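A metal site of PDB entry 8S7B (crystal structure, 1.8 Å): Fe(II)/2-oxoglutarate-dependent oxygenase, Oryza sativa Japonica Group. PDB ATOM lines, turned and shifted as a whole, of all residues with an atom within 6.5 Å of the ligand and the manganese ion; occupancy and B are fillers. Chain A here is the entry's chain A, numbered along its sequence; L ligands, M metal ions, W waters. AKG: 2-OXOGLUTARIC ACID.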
ATOM      1  N   ARG A 212       3.098 -32.477  19.897  1.00  0.00           N
ATOM      2  CA  ARG A 212       1.789 -31.919  20.219  1.00  0.00           C
ATOM      3  C   ARG A 212       0.975 -31.837  18.942  1.00  0.00           C
ATOM      4  O   ARG A 212       1.214 -30.965  18.099  1.00  0.00           O
ATOM      5  CB  ARG A 212       1.909 -30.541  20.889  1.00  0.00           C
ATOM      6  CG  ARG A 212       0.572 -29.954  21.350  1.00  0.00           C
ATOM      7  CD  ARG A 212       0.745 -28.560  21.995  1.00  0.00           C
ATOM      8  NE  ARG A 212      -0.562 -27.973  22.298  1.00  0.00           N
ATOM      9  CZ  ARG A 212      -1.065 -27.817  23.509  1.00  0.00           C
ATOM     10  NH1 ARG A 212      -0.371 -28.105  24.593  1.00  0.00           N
ATOM     11  NH2 ARG A 212      -2.312 -27.370  23.638  1.00  0.00           N
ATOM     12  N   ASN A 214      -2.172 -30.641  17.526  1.00  0.00           N
ATOM     13  CA  ASN A 214      -3.281 -29.736  17.792  1.00  0.00           C
ATOM     14  C   ASN A 214      -4.433 -29.976  16.825  1.00  0.00           C
ATOM     15  O   ASN A 214      -4.215 -30.174  15.622  1.00  0.00           O
ATOM     16  CB  ASN A 214      -2.837 -28.279  17.673  1.00  0.00           C
ATOM     17  CG  ASN A 214      -1.776 -27.916  18.687  1.00  0.00           C
ATOM     18  OD1 ASN A 214      -2.051 -27.850  19.882  1.00  0.00           O
ATOM     19  ND2 ASN A 214      -0.552 -27.683  18.205  1.00  0.00           N
ATOM     20  N   TYR A 216      -7.979 -27.934  15.925  1.00  0.00           N
ATOM     21  CA  TYR A 216      -8.817 -26.752  16.109  1.00  0.00           C
ATOM     22  C   TYR A 216     -10.132 -26.963  15.380  1.00  0.00           C
ATOM     23  O   TYR A 216     -10.183 -26.820  14.146  1.00  0.00           O
ATOM     24  CB  TYR A 216      -8.098 -25.507  15.590  1.00  0.00           C
ATOM     25  CG  TYR A 216      -6.696 -25.330  16.131  1.00  0.00           C
ATOM     26  CD1 TYR A 216      -6.477 -24.650  17.326  1.00  0.00           C
ATOM     27  CD2 TYR A 216      -5.597 -25.847  15.461  1.00  0.00           C
ATOM     28  CE1 TYR A 216      -5.207 -24.501  17.846  1.00  0.00           C
ATOM     29  CE2 TYR A 216      -4.304 -25.689  15.966  1.00  0.00           C
ATOM     30  CZ  TYR A 216      -4.119 -25.022  17.158  1.00  0.00           C
ATOM     31  OH  TYR A 216      -2.865 -24.855  17.684  1.00  0.00           O
ATOM     32  N   ILE A 228      -5.615 -21.489  20.082  1.00  0.00           N
ATOM     33  CA  ILE A 228      -4.678 -21.582  21.201  1.00  0.00           C
ATOM     34  C   ILE A 228      -4.290 -20.173  21.594  1.00  0.00           C
ATOM     35  O   ILE A 228      -4.077 -19.307  20.731  1.00  0.00           O
ATOM     36  CB  ILE A 228      -3.445 -22.467  20.865  1.00  0.00           C
ATOM     37  CG1 ILE A 228      -2.629 -22.731  22.137  1.00  0.00           C
ATOM     38  CG2 ILE A 228      -2.573 -21.855  19.779  1.00  0.00           C
ATOM     39  CD1 ILE A 228      -1.538 -23.786  21.944  1.00  0.00           C
ATOM     40  N   HIS A 231       0.877 -17.150  23.345  1.00  0.00           N
ATOM     41  CA  HIS A 231       1.876 -17.757  24.197  1.00  0.00           C
ATOM     42  C   HIS A 231       3.199 -17.755  23.453  1.00  0.00           C
ATOM     43  O   HIS A 231       3.243 -17.681  22.226  1.00  0.00           O
ATOM     44  CB  HIS A 231       1.492 -19.185  24.582  1.00  0.00           C
ATOM     45  CG  HIS A 231       1.565 -20.159  23.441  1.00  0.00           C
ATOM     46  ND1 HIS A 231       0.569 -20.271  22.492  1.00  0.00           N
ATOM     47  CD2 HIS A 231       2.528 -21.044  23.087  1.00  0.00           C
ATOM     48  CE1 HIS A 231       0.917 -21.190  21.608  1.00  0.00           C
ATOM     49  NE2 HIS A 231       2.100 -21.665  21.936  1.00  0.00           N
ATOM     50  N   SER A 232       4.277 -17.814  24.227  1.00  0.00           N
ATOM     51  CA  SER A 232       5.551 -18.243  23.707  1.00  0.00           C
ATOM     52  C   SER A 232       5.780 -19.677  24.159  1.00  0.00           C
ATOM     53  O   SER A 232       5.322 -20.081  25.237  1.00  0.00           O
ATOM     54  CB  SER A 232       6.693 -17.342  24.184  1.00  0.00           C
ATOM     55  OG  SER A 232       6.776 -17.338  25.599  1.00  0.00           O
ATOM     56  N   ASP A 233       6.458 -20.464  23.325  1.00  0.00           N
ATOM     57  CA  ASP A 233       6.790 -21.816  23.732  1.00  0.00           C
ATOM     58  C   ASP A 233       7.854 -21.787  24.824  1.00  0.00           C
ATOM     59  O   ASP A 233       8.717 -20.900  24.860  1.00  0.00           O
ATOM     60  CB  ASP A 233       7.284 -22.641  22.543  1.00  0.00           C
ATOM     61  CG  ASP A 233       6.201 -22.873  21.495  1.00  0.00           C
ATOM     62  OD1 ASP A 233       5.005 -22.636  21.782  1.00  0.00           O
ATOM     63  OD2 ASP A 233       6.546 -23.310  20.378  1.00  0.00           O
ATOM     64  N   THR A 238      11.215 -25.151  18.775  1.00  0.00           N
ATOM     65  CA  THR A 238      10.018 -25.838  18.317  1.00  0.00           C
ATOM     66  C   THR A 238      10.061 -25.952  16.804  1.00  0.00           C
ATOM     67  O   THR A 238      10.419 -24.996  16.105  1.00  0.00           O
ATOM     68  CB  THR A 238       8.749 -25.105  18.755  1.00  0.00           C
ATOM     69  OG1 THR A 238       8.690 -25.036  20.186  1.00  0.00           O
ATOM     70  CG2 THR A 238       7.483 -25.828  18.236  1.00  0.00           C
ATOM     71  N   LEU A 240       7.561 -26.790  13.772  1.00  0.00           N
ATOM     72  CA  LEU A 240       6.110 -26.802  13.617  1.00  0.00           C
ATOM     73  C   LEU A 240       5.723 -27.121  12.181  1.00  0.00           C
ATOM     74  O   LEU A 240       6.269 -26.534  11.236  1.00  0.00           O
ATOM     75  CB  LEU A 240       5.518 -25.447  14.027  1.00  0.00           C
ATOM     76  CG  LEU A 240       4.008 -25.246  13.921  1.00  0.00           C
ATOM     77  CD1 LEU A 240       3.293 -26.095  14.936  1.00  0.00           C
ATOM     78  CD2 LEU A 240       3.649 -23.768  14.111  1.00  0.00           C
ATOM     79  N   LEU A 241       4.757 -28.024  12.025  1.00  0.00           N
ATOM     80  CA  LEU A 241       4.196 -28.381  10.721  1.00  0.00           C
ATOM     81  C   LEU A 241       2.715 -28.005  10.753  1.00  0.00           C
ATOM     82  O   LEU A 241       1.945 -28.598  11.521  1.00  0.00           O
ATOM     83  CB  LEU A 241       4.384 -29.868  10.429  1.00  0.00           C
ATOM     84  CG  LEU A 241       3.839 -30.416   9.118  1.00  0.00           C
ATOM     85  CD1 LEU A 241       4.279 -29.569   7.929  1.00  0.00           C
ATOM     86  CD2 LEU A 241       4.272 -31.874   8.953  1.00  0.00           C
ATOM     87  N   VAL A 242       2.321 -27.020   9.949  1.00  0.00           N
ATOM     88  CA  VAL A 242       0.971 -26.483  10.017  1.00  0.00           C
ATOM     89  C   VAL A 242       0.104 -27.111   8.933  1.00  0.00           C
ATOM     90  O   VAL A 242       0.589 -27.628   7.916  1.00  0.00           O
ATOM     91  CB  VAL A 242       0.933 -24.944   9.895  1.00  0.00           C
ATOM     92  CG1 VAL A 242       1.666 -24.295  11.056  1.00  0.00           C
ATOM     93  CG2 VAL A 242       1.524 -24.495   8.575  1.00  0.00           C
ATOM     94  N   ASP A 243      -1.198 -27.097   9.184  1.00  0.00           N
ATOM     95  CA  ASP A 243      -2.214 -27.400   8.192  1.00  0.00           C
ATOM     96  C   ASP A 243      -1.881 -26.743   6.857  1.00  0.00           C
ATOM     97  O   ASP A 243      -1.598 -25.545   6.803  1.00  0.00           O
ATOM     98  CB  ASP A 243      -3.569 -26.887   8.697  1.00  0.00           C
ATOM     99  CG  ASP A 243      -4.754 -27.560   8.047  1.00  0.00           C
ATOM    100  OD1 ASP A 243      -4.884 -27.529   6.804  1.00  0.00           O
ATOM    101  OD2 ASP A 243      -5.567 -28.121   8.807  1.00  0.00           O
ATOM    102  N   GLY A 248      -4.500 -19.816  10.206  1.00  0.00           N
ATOM    103  CA  GLY A 248      -4.881 -19.527  11.572  1.00  0.00           C
ATOM    104  C   GLY A 248      -3.743 -19.125  12.482  1.00  0.00           C
ATOM    105  O   GLY A 248      -3.954 -18.445  13.484  1.00  0.00           O
ATOM    106  N   LEU A 249      -2.526 -19.551  12.157  1.00  0.00           N
ATOM    107  CA  LEU A 249      -1.372 -19.172  12.966  1.00  0.00           C
ATOM    108  C   LEU A 249      -1.065 -17.687  12.795  1.00  0.00           C
ATOM    109  O   LEU A 249      -1.041 -17.169  11.672  1.00  0.00           O
ATOM    110  CB  LEU A 249      -0.156 -20.007  12.580  1.00  0.00           C
ATOM    111  CG  LEU A 249       1.159 -19.701  13.287  1.00  0.00           C
ATOM    112  CD1 LEU A 249       1.046 -19.925  14.790  1.00  0.00           C
ATOM    113  CD2 LEU A 249       2.289 -20.541  12.704  1.00  0.00           C
ATOM    114  N   LEU A 268       8.111 -24.592   9.944  1.00  0.00           N
ATOM    115  CA  LEU A 268       8.272 -23.375  10.729  1.00  0.00           C
ATOM    116  C   LEU A 268       9.088 -23.692  11.971  1.00  0.00           C
ATOM    117  O   LEU A 268       8.740 -24.596  12.733  1.00  0.00           O
ATOM    118  CB  LEU A 268       6.923 -22.784  11.121  1.00  0.00           C
ATOM    119  CG  LEU A 268       6.182 -22.030  10.023  1.00  0.00           C
ATOM    120  CD1 LEU A 268       4.676 -22.037  10.302  1.00  0.00           C
ATOM    121  CD2 LEU A 268       6.699 -20.616  10.003  1.00  0.00           C
ATOM    122  N   ASN A 270      10.694 -22.028  15.495  1.00  0.00           N
ATOM    123  CA  ASN A 270      10.726 -20.885  16.404  1.00  0.00           C
ATOM    124  C   ASN A 270      11.530 -21.254  17.639  1.00  0.00           C
ATOM    125  O   ASN A 270      11.540 -22.404  18.080  1.00  0.00           O
ATOM    126  CB  ASN A 270       9.313 -20.409  16.825  1.00  0.00           C
ATOM    127  CG  ASN A 270       8.518 -21.473  17.572  1.00  0.00           C
ATOM    128  OD1 ASN A 270       7.946 -22.368  16.960  1.00  0.00           O
ATOM    129  ND2 ASN A 270       8.450 -21.340  18.897  1.00  0.00           N
ATOM    130  N   HIS A 288       2.897 -16.218  19.892  1.00  0.00           N
ATOM    131  CA  HIS A 288       2.068 -16.587  18.765  1.00  0.00           C
ATOM    132  C   HIS A 288       0.724 -17.101  19.270  1.00  0.00           C
ATOM    133  O   HIS A 288       0.550 -17.361  20.466  1.00  0.00           O
ATOM    134  CB  HIS A 288       2.751 -17.645  17.881  1.00  0.00           C
ATOM    135  CG  HIS A 288       3.272 -18.821  18.653  1.00  0.00           C
ATOM    136  ND1 HIS A 288       4.430 -18.781  19.392  1.00  0.00           N
ATOM    137  CD2 HIS A 288       2.779 -20.076  18.796  1.00  0.00           C
ATOM    138  CE1 HIS A 288       4.638 -19.960  19.955  1.00  0.00           C
ATOM    139  NE2 HIS A 288       3.645 -20.769  19.612  1.00  0.00           N
ATOM    140  N   ARG A 289      -0.218 -17.230  18.352  1.00  0.00           N
ATOM    141  CA  ARG A 289      -1.561 -17.712  18.694  1.00  0.00           C
ATOM    142  C   ARG A 289      -2.175 -18.334  17.443  1.00  0.00           C
ATOM    143  O   ARG A 289      -1.650 -18.216  16.340  1.00  0.00           O
ATOM    144  CB  ARG A 289      -2.447 -16.575  19.223  1.00  0.00           C
ATOM    145  CG  ARG A 289      -2.872 -15.589  18.137  1.00  0.00           C
ATOM    146  CD  ARG A 289      -3.531 -14.346  18.701  1.00  0.00           C
ATOM    147  NE  ARG A 289      -4.012 -13.471  17.639  1.00  0.00           N
ATOM    148  CZ  ARG A 289      -4.553 -12.280  17.848  1.00  0.00           C
ATOM    149  NH1 ARG A 289      -4.708 -11.788  19.065  1.00  0.00           N
ATOM    150  NH2 ARG A 289      -4.950 -11.565  16.801  1.00  0.00           N
ATOM    151  N   VAL A 290      -3.309 -19.003  17.632  1.00  0.00           N
ATOM    152  CA  VAL A 290      -4.089 -19.507  16.502  1.00  0.00           C
ATOM    153  C   VAL A 290      -5.501 -18.989  16.656  1.00  0.00           C
ATOM    154  O   VAL A 290      -6.099 -19.111  17.724  1.00  0.00           O
ATOM    155  CB  VAL A 290      -4.079 -21.043  16.422  1.00  0.00           C
ATOM    156  CG1 VAL A 290      -5.072 -21.538  15.377  1.00  0.00           C
ATOM    157  CG2 VAL A 290      -2.679 -21.533  16.086  1.00  0.00           C
ATOM    158  N   ARG A 298      -8.742 -27.336  11.647  1.00  0.00           N
ATOM    159  CA  ARG A 298      -7.338 -27.095  11.353  1.00  0.00           C
ATOM    160  C   ARG A 298      -6.491 -27.977  12.257  1.00  0.00           C
ATOM    161  O   ARG A 298      -6.816 -28.155  13.429  1.00  0.00           O
ATOM    162  CB  ARG A 298      -6.964 -25.616  11.565  1.00  0.00           C
ATOM    163  CG  ARG A 298      -5.491 -25.276  11.312  1.00  0.00           C
ATOM    164  CD  ARG A 298      -5.198 -23.799  11.590  1.00  0.00           C
ATOM    165  NE  ARG A 298      -3.785 -23.463  11.359  1.00  0.00           N
ATOM    166  CZ  ARG A 298      -2.825 -23.634  12.248  1.00  0.00           C
ATOM    167  NH1 ARG A 298      -3.086 -24.104  13.461  1.00  0.00           N
ATOM    168  NH2 ARG A 298      -1.569 -23.340  11.918  1.00  0.00           N
ATOM    169  N   ILE A 299      -5.409 -28.538  11.721  1.00  0.00           N
ATOM    170  CA  ILE A 299      -4.507 -29.350  12.522  1.00  0.00           C
ATOM    171  C   ILE A 299      -3.093 -28.802  12.409  1.00  0.00           C
ATOM    172  O   ILE A 299      -2.747 -28.125  11.431  1.00  0.00           O
ATOM    173  CB  ILE A 299      -4.529 -30.838  12.096  1.00  0.00           C
ATOM    174  CG1 ILE A 299      -4.167 -30.977  10.620  1.00  0.00           C
ATOM    175  CG2 ILE A 299      -5.889 -31.470  12.404  1.00  0.00           C
ATOM    176  CD1 ILE A 299      -3.568 -32.329  10.258  1.00  0.00           C
ATOM    177  N   SER A 300      -2.291 -29.063  13.426  1.00  0.00           N
ATOM    178  CA  SER A 300      -0.856 -28.790  13.356  1.00  0.00           C
ATOM    179  C   SER A 300      -0.147 -29.820  14.220  1.00  0.00           C
ATOM    180  O   SER A 300      -0.756 -30.466  15.079  1.00  0.00           O
ATOM    181  CB  SER A 300      -0.516 -27.375  13.830  1.00  0.00           C
ATOM    182  OG  SER A 300      -0.750 -27.254  15.222  1.00  0.00           O
ATOM    183  N   LEU A 301       1.154 -29.979  13.978  1.00  0.00           N
ATOM    184  CA  LEU A 301       2.017 -30.845  14.767  1.00  0.00           C
ATOM    185  C   LEU A 301       3.234 -30.035  15.193  1.00  0.00           C
ATOM    186  O   LEU A 301       4.031 -29.624  14.346  1.00  0.00           O
ATOM    187  CB  LEU A 301       2.443 -32.088  13.983  1.00  0.00           C
ATOM    188  CG  LEU A 301       3.546 -32.929  14.635  1.00  0.00           C
ATOM    189  CD1 LEU A 301       3.174 -33.346  16.065  1.00  0.00           C
ATOM    190  CD2 LEU A 301       3.875 -34.168  13.786  1.00  0.00           C
ATOM    191  N   ALA A 302       3.367 -29.816  16.487  1.00  0.00           N
ATOM    192  CA  ALA A 302       4.529 -29.118  17.044  1.00  0.00           C
ATOM    193  C   ALA A 302       5.454 -30.138  17.693  1.00  0.00           C
ATOM    194  O   ALA A 302       5.036 -30.868  18.594  1.00  0.00           O
ATOM    195  CB  ALA A 302       4.083 -28.074  18.076  1.00  0.00           C
ATOM    196  N   LEU A 304       8.307 -30.317  20.140  1.00  0.00           N
ATOM    197  CA  LEU A 304       8.718 -29.434  21.227  1.00  0.00           C
ATOM    198  C   LEU A 304       9.985 -29.995  21.847  1.00  0.00           C
ATOM    199  O   LEU A 304       9.947 -31.048  22.492  1.00  0.00           O
ATOM    200  CB  LEU A 304       7.599 -29.326  22.264  1.00  0.00           C
ATOM    201  CG  LEU A 304       6.267 -28.823  21.721  1.00  0.00           C
ATOM    202  CD1 LEU A 304       5.114 -29.219  22.653  1.00  0.00           C
ATOM    203  CD2 LEU A 304       6.310 -27.306  21.538  1.00  0.00           C
HETATM  204  C1  AKG L   1       1.969 -25.029  19.927  1.00  0.00           C
HETATM  205  O1  AKG L   1       2.724 -24.651  20.825  1.00  0.00           O
HETATM  206  O2  AKG L   1       1.508 -26.245  19.790  1.00  0.00           O
HETATM  207  C2  AKG L   1       1.499 -24.055  18.861  1.00  0.00           C
HETATM  208  O5  AKG L   1       1.762 -22.868  18.993  1.00  0.00           O
HETATM  209  C3  AKG L   1       0.720 -24.583  17.683  1.00  0.00           C
HETATM  210  C4  AKG L   1       0.575 -23.559  16.578  1.00  0.00           C
HETATM  211  C5  AKG L   1      -0.307 -24.007  15.443  1.00  0.00           C
HETATM  212  O3  AKG L   1      -1.281 -24.724  15.579  1.00  0.00           O
HETATM  213  O4  AKG L   1       0.073 -23.514  14.285  1.00  0.00           O
HETATM  214 MN    MN M   1       3.294 -22.686  20.469  1.00  0.00          MN
HETATM  215  O   HOH W   1       4.540 -23.514  18.726  1.00  0.00           O
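ND2 of Asn 214 sits at hydrogen-bond distance from O2 of the ligand (3.0 Å).
The guanidinium group of Arg 212 is in salt-bridge range of an oxygen (O2) of the ligand (3.7 Å).
The side-chain hydroxyl of Ser 300 is in hydrogen-bond range of an oxygen (O3) of the ligand.
The guanidinium group of Arg 298 is in salt-bridge range of an oxygen (O3) of the ligand (2.9 Å).
The side-chain hydroxyl (OH) of Tyr 216 is in hydrogen-bond range of an oxygen (O3) of the ligand (2.6 Å).
The backbone carbonyl oxygen (O) of Ala 302 is in hydrogen-bond range of the backbone NH (N) of Arg 212 (2.8 Å).
OD2 of Asp 233 lies within hydrogen-bond range of ND2 of Asn 270 (3.1 Å).
The backbone NH of Leu 240 lies within hydrogen-bond range of the backbone carbonyl oxygen of Leu 268 (2.7 Å).
OG1 of Thr 238 is in hydrogen-bond range of OD2 of Asp 233 (2.8 Å).
OD1 of Asn 214 is in hydrogen-bond range of NE of Arg 212, at 2.8 Å.
O of Arg 298 sits at hydrogen-bond distance from N of Tyr 216 (2.8 Å).
N of Asn 214 lies within hydrogen-bond range of O of Ser 300, 2.8 Å away.
N of Val 290 lies within hydrogen-bond range of O of Ile 228.
Leu 240 touches the ligand.
Val 242 touches the ligand (CG1 to O4, 3.7 Å).
Leu 249 touches the ligand (CD1 to O4, 3.8 Å).
Val 290 touches the ligand.
Ala 302 touches the ligand (CB to O2, 3.6 Å).
Hydrophobic or aromatic side chains within 4 Å of the ligand: Tyr 216, His 231, Leu 240, Val 242, Leu 249, His 288, Val 290 and Ala 302.
13 residues have an atom within 4 Å of the ligand: Arg 212, Asn 214, Tyr 216, His 231, Asp 233, Leu 240, Val 242, Leu 249, His 288, Val 290, Arg 298, Ser 300 and Ala 302.
Along chain A the residues within 4 Å of the ligand span positions 212 to 302.
The nearest printed residue that does not touch the ligand is Ile 228 (4.2 Å).
Of the 25 residues printed, 3 come within 4 Å of the manganese ion.
O1 of the ligand binds the manganese ion.
NE2 of His 288 binds the manganese ion (2.1 Å).
The manganese ion is bound by an oxygen (O5) of the ligand (2.1 Å).
NE2 of His 231 binds the manganese ion (2.1 Å).
The manganese ion is bound by OD1 of Asp 233, at 2.2 Å.
Water W1 is bound to the manganese ion, 2.3 Å away.
The manganese ion has six donor atoms within binding distance.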
